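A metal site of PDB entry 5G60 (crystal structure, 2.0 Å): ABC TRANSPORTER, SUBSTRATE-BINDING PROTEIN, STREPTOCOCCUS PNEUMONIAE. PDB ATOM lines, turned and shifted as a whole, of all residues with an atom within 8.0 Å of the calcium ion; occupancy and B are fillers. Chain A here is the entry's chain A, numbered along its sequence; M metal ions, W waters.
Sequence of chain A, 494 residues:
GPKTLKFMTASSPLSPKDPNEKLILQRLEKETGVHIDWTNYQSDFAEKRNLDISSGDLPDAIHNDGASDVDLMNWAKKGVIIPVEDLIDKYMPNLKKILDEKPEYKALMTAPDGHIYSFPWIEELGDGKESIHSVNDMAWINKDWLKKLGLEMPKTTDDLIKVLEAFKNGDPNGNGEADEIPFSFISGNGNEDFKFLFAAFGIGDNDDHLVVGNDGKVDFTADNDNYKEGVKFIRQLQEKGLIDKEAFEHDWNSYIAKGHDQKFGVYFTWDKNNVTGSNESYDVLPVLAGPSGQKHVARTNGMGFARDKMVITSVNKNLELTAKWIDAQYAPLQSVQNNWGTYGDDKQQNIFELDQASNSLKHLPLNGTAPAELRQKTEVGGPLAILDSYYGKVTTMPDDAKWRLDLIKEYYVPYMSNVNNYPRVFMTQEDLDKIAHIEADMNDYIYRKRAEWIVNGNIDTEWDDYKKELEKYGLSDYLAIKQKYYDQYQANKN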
ATOM      1  N   ILE A 203      -6.745  34.051  31.671  1.00  0.00           N
ATOM      2  CA  ILE A 203      -7.704  33.001  31.348  1.00  0.00           C
ATOM      3  C   ILE A 203      -7.596  31.733  32.215  1.00  0.00           C
ATOM      4  O   ILE A 203      -8.587  31.367  32.928  1.00  0.00           O
ATOM      5  CB  ILE A 203      -7.722  32.631  29.860  1.00  0.00           C
ATOM      6  CG1 ILE A 203      -7.822  33.921  29.059  1.00  0.00           C
ATOM      7  CG2 ILE A 203      -8.868  31.661  29.600  1.00  0.00           C
ATOM      8  CD1 ILE A 203      -7.902  33.762  27.577  1.00  0.00           C
ATOM      9  N   HIS A 209     -11.170  22.143  30.753  1.00  0.00           N
ATOM     10  CA  HIS A 209     -10.489  23.004  29.800  1.00  0.00           C
ATOM     11  C   HIS A 209     -11.487  23.940  29.073  1.00  0.00           C
ATOM     12  O   HIS A 209     -11.311  24.202  27.877  1.00  0.00           O
ATOM     13  CB  HIS A 209      -9.643  22.204  28.766  1.00  0.00           C
ATOM     14  CG  HIS A 209      -8.760  21.182  29.377  1.00  0.00           C
ATOM     15  ND1 HIS A 209      -7.795  21.502  30.304  1.00  0.00           N
ATOM     16  CD2 HIS A 209      -8.754  19.832  29.280  1.00  0.00           C
ATOM     17  CE1 HIS A 209      -7.245  20.392  30.759  1.00  0.00           C
ATOM     18  NE2 HIS A 209      -7.769  19.368  30.121  1.00  0.00           N
ATOM     19  N   LEU A 210     -12.463  24.470  29.822  1.00  0.00           N
ATOM     20  CA  LEU A 210     -13.592  25.172  29.211  1.00  0.00           C
ATOM     21  C   LEU A 210     -14.016  26.245  30.157  1.00  0.00           C
ATOM     22  O   LEU A 210     -14.367  25.965  31.296  1.00  0.00           O
ATOM     23  CB  LEU A 210     -14.732  24.201  28.943  1.00  0.00           C
ATOM     24  CG  LEU A 210     -15.746  24.631  27.907  1.00  0.00           C
ATOM     25  CD1 LEU A 210     -15.141  24.531  26.511  1.00  0.00           C
ATOM     26  CD2 LEU A 210     -16.994  23.764  27.962  1.00  0.00           C
ATOM     27  N   VAL A 211     -13.883  27.481  29.728  1.00  0.00           N
ATOM     28  CA  VAL A 211     -14.427  28.616  30.412  1.00  0.00           C
ATOM     29  C   VAL A 211     -15.431  29.362  29.524  1.00  0.00           C
ATOM     30  O   VAL A 211     -15.567  29.069  28.355  1.00  0.00           O
ATOM     31  CB  VAL A 211     -13.339  29.547  30.947  1.00  0.00           C
ATOM     32  CG1 VAL A 211     -12.472  28.839  32.003  1.00  0.00           C
ATOM     33  CG2 VAL A 211     -12.476  30.116  29.838  1.00  0.00           C
ATOM     34  N   VAL A 218     -17.912  30.412  24.599  1.00  0.00           N
ATOM     35  CA  VAL A 218     -17.221  29.291  25.289  1.00  0.00           C
ATOM     36  C   VAL A 218     -15.764  29.255  24.813  1.00  0.00           C
ATOM     37  O   VAL A 218     -15.540  29.348  23.623  1.00  0.00           O
ATOM     38  CB  VAL A 218     -17.964  27.965  24.972  1.00  0.00           C
ATOM     39  CG1 VAL A 218     -17.289  26.804  25.617  1.00  0.00           C
ATOM     40  CG2 VAL A 218     -19.389  28.006  25.510  1.00  0.00           C
ATOM     41  N   ASP A 219     -14.777  29.161  25.703  1.00  0.00           N
ATOM     42  CA  ASP A 219     -13.395  29.307  25.250  1.00  0.00           C
ATOM     43  C   ASP A 219     -12.573  28.022  25.364  1.00  0.00           C
ATOM     44  O   ASP A 219     -12.732  27.420  26.484  1.00  0.00           O
ATOM     45  CB  ASP A 219     -12.689  30.329  26.116  1.00  0.00           C
ATOM     46  CG  ASP A 219     -11.232  30.466  25.785  1.00  0.00           C
ATOM     47  OD1 ASP A 219     -10.746  29.872  24.808  1.00  0.00           O
ATOM     48  OD2 ASP A 219     -10.510  31.186  26.495  1.00  0.00           O
ATOM     49  N   PHE A 220     -11.554  27.737  24.431  1.00  0.00           N
ATOM     50  CA  PHE A 220     -11.071  26.414  24.770  1.00  0.00           C
ATOM     51  C   PHE A 220      -9.737  26.923  25.200  1.00  0.00           C
ATOM     52  O   PHE A 220      -8.843  27.123  24.585  1.00  0.00           O
ATOM     53  CB  PHE A 220     -11.181  25.272  23.754  1.00  0.00           C
ATOM     54  CG  PHE A 220     -10.473  23.996  24.134  1.00  0.00           C
ATOM     55  CD1 PHE A 220     -11.099  22.999  24.840  1.00  0.00           C
ATOM     56  CD2 PHE A 220      -9.172  23.764  23.674  1.00  0.00           C
ATOM     57  CE1 PHE A 220     -10.431  21.804  25.130  1.00  0.00           C
ATOM     58  CE2 PHE A 220      -8.521  22.571  23.950  1.00  0.00           C
ATOM     59  CZ  PHE A 220      -9.155  21.589  24.675  1.00  0.00           C
ATOM     60  N   THR A 221      -9.641  26.447  26.488  1.00  0.00           N
ATOM     61  CA  THR A 221      -8.475  26.874  27.317  1.00  0.00           C
ATOM     62  C   THR A 221      -7.124  26.325  26.868  1.00  0.00           C
ATOM     63  O   THR A 221      -6.103  27.043  26.897  1.00  0.00           O
ATOM     64  CB  THR A 221      -8.577  26.728  28.833  1.00  0.00           C
ATOM     65  OG1 THR A 221      -8.676  25.360  29.189  1.00  0.00           O
ATOM     66  CG2 THR A 221      -9.782  27.544  29.401  1.00  0.00           C
ATOM     67  N   ALA A 222      -7.123  25.044  26.507  1.00  0.00           N
ATOM     68  CA  ALA A 222      -5.858  24.315  26.316  1.00  0.00           C
ATOM     69  C   ALA A 222      -5.212  24.557  24.913  1.00  0.00           C
ATOM     70  O   ALA A 222      -4.156  23.968  24.610  1.00  0.00           O
ATOM     71  CB  ALA A 222      -6.083  22.819  26.564  1.00  0.00           C
ATOM     72  N   ASP A 223      -5.842  25.412  24.110  1.00  0.00           N
ATOM     73  CA  ASP A 223      -5.244  25.983  22.911  1.00  0.00           C
ATOM     74  C   ASP A 223      -4.890  27.476  23.001  1.00  0.00           C
ATOM     75  O   ASP A 223      -4.555  28.102  21.987  1.00  0.00           O
ATOM     76  CB  ASP A 223      -6.110  25.661  21.681  1.00  0.00           C
ATOM     77  CG  ASP A 223      -7.410  26.441  21.612  1.00  0.00           C
ATOM     78  OD1 ASP A 223      -7.855  27.133  22.559  1.00  0.00           O
ATOM     79  OD2 ASP A 223      -8.034  26.318  20.557  1.00  0.00           O
ATOM     80  N   ASN A 224      -4.918  28.070  24.201  1.00  0.00           N
ATOM     81  CA  ASN A 224      -4.717  29.537  24.228  1.00  0.00           C
ATOM     82  C   ASN A 224      -3.261  29.892  24.365  1.00  0.00           C
ATOM     83  O   ASN A 224      -2.558  29.238  25.100  1.00  0.00           O
ATOM     84  CB  ASN A 224      -5.477  30.156  25.372  1.00  0.00           C
ATOM     85  CG  ASN A 224      -7.009  30.086  25.209  1.00  0.00           C
ATOM     86  OD1 ASN A 224      -7.611  29.788  24.127  1.00  0.00           O
ATOM     87  ND2 ASN A 224      -7.663  30.311  26.352  1.00  0.00           N
ATOM     88  N   ASP A 225      -2.799  30.961  23.751  1.00  0.00           N
ATOM     89  CA  ASP A 225      -1.457  31.409  24.043  1.00  0.00           C
ATOM     90  C   ASP A 225      -1.192  31.517  25.558  1.00  0.00           C
ATOM     91  O   ASP A 225      -0.111  31.194  26.077  1.00  0.00           O
ATOM     92  CB  ASP A 225      -1.151  32.751  23.394  1.00  0.00           C
ATOM     93  CG  ASP A 225      -1.010  32.657  21.870  1.00  0.00           C
ATOM     94  OD1 ASP A 225      -0.916  31.560  21.295  1.00  0.00           O
ATOM     95  OD2 ASP A 225      -1.000  33.709  21.256  1.00  0.00           O
ATOM     96  N   ASN A 226      -2.183  31.981  26.278  1.00  0.00           N
ATOM     97  CA  ASN A 226      -2.075  32.055  27.741  1.00  0.00           C
ATOM     98  C   ASN A 226      -1.721  30.720  28.362  1.00  0.00           C
ATOM     99  O   ASN A 226      -0.981  30.669  29.349  1.00  0.00           O
ATOM    100  CB  ASN A 226      -3.411  32.495  28.352  1.00  0.00           C
ATOM    101  CG  ASN A 226      -3.973  33.717  27.674  1.00  0.00           C
ATOM    102  OD1 ASN A 226      -4.507  33.627  26.582  1.00  0.00           O
ATOM    103  ND2 ASN A 226      -3.783  34.854  28.285  1.00  0.00           N
ATOM    104  N   TYR A 227      -2.320  29.656  27.835  1.00  0.00           N
ATOM    105  CA  TYR A 227      -2.067  28.316  28.342  1.00  0.00           C
ATOM    106  C   TYR A 227      -0.614  27.885  28.021  1.00  0.00           C
ATOM    107  O   TYR A 227       0.105  27.321  28.859  1.00  0.00           O
ATOM    108  CB  TYR A 227      -3.082  27.374  27.712  1.00  0.00           C
ATOM    109  CG  TYR A 227      -2.972  25.906  28.098  1.00  0.00           C
ATOM    110  CD1 TYR A 227      -2.126  25.033  27.389  1.00  0.00           C
ATOM    111  CD2 TYR A 227      -3.767  25.377  29.104  1.00  0.00           C
ATOM    112  CE1 TYR A 227      -2.024  23.665  27.721  1.00  0.00           C
ATOM    113  CE2 TYR A 227      -3.682  23.998  29.449  1.00  0.00           C
ATOM    114  CZ  TYR A 227      -2.816  23.145  28.753  1.00  0.00           C
ATOM    115  OH  TYR A 227      -2.743  21.827  29.095  1.00  0.00           O
ATOM    116  N   LYS A 467      -2.043  22.209  18.060  1.00  0.00           N
ATOM    117  CA  LYS A 467      -3.349  22.798  17.756  1.00  0.00           C
ATOM    118  C   LYS A 467      -3.954  22.170  16.544  1.00  0.00           C
ATOM    119  O   LYS A 467      -5.156  21.910  16.541  1.00  0.00           O
ATOM    120  CB  LYS A 467      -3.302  24.324  17.608  1.00  0.00           C
ATOM    121  CG  LYS A 467      -2.957  25.037  18.890  1.00  0.00           C
ATOM    122  CD  LYS A 467      -3.286  26.519  18.840  1.00  0.00           C
ATOM    123  CE  LYS A 467      -2.284  27.252  17.944  1.00  0.00           C
ATOM    124  NZ  LYS A 467      -2.541  28.704  18.052  1.00  0.00           N
ATOM    125  N   LEU A 475     -11.965  19.377  17.705  1.00  0.00           N
ATOM    126  CA  LEU A 475     -12.139  20.479  18.611  1.00  0.00           C
ATOM    127  C   LEU A 475     -13.225  21.488  18.162  1.00  0.00           C
ATOM    128  O   LEU A 475     -14.046  21.913  18.966  1.00  0.00           O
ATOM    129  CB  LEU A 475     -10.789  21.156  18.870  1.00  0.00           C
ATOM    130  CG  LEU A 475     -10.822  22.357  19.808  1.00  0.00           C
ATOM    131  CD1 LEU A 475     -11.488  22.036  21.142  1.00  0.00           C
ATOM    132  CD2 LEU A 475      -9.409  22.880  19.969  1.00  0.00           C
ATOM    133  N   LEU A 479     -16.520  22.489  20.259  1.00  0.00           N
ATOM    134  CA  LEU A 479     -16.864  23.826  20.769  1.00  0.00           C
ATOM    135  C   LEU A 479     -18.213  24.275  20.322  1.00  0.00           C
ATOM    136  O   LEU A 479     -19.005  24.772  21.127  1.00  0.00           O
ATOM    137  CB  LEU A 479     -15.833  24.862  20.354  1.00  0.00           C
ATOM    138  CG  LEU A 479     -14.597  24.839  21.235  1.00  0.00           C
ATOM    139  CD1 LEU A 479     -13.617  25.899  20.728  1.00  0.00           C
ATOM    140  CD2 LEU A 479     -14.948  25.060  22.711  1.00  0.00           C
HETATM  141 CA    CA M   1      -9.467  28.752  23.245  1.00  0.00          CA
HETATM  142  O   HOH W   1     -11.345  28.060  22.168  1.00  0.00           O
HETATM  143  O   HOH W   2      -9.730  31.007  22.426  1.00  0.00           O
HETATM  144  O   HOH W   3      -8.553  29.348  21.123  1.00  0.00           O
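Merely in contact with the calcium ion: Thr 221 (3.98 Å). Within 4 Å of the calcium ion: Asp 219, Phe 220, Thr 221, Asp 223 and Asn 224. The nearest printed residue that does not touch the calcium ion is Ala 222 (5.5 Å).
The backbone NH of Thr 221 lies within hydrogen-bond range of the backbone carbonyl oxygen of His 209, at 3.1 Å. The backbone carbonyl oxygen (O) of Val 211 sits at hydrogen-bond distance from the backbone NH (N) of Asp 219 (2.8 Å).
O of Phe 220 is bound to the calcium ion. Water W1 is bound to the calcium ion. The calcium ion is bound by OD1 of Asn 224. The side-chain carboxylate (OD1) of Asp 219 binds the calcium ion. The calcium ion is bound by OD1 of Asp 223 (2.4 Å). The calcium ion is bound by water W3. The calcium ion is bound by water W2. The calcium ion is bound by N of Phe 220 (2.6 Å). The calcium ion has eight donor atoms within binding distance.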
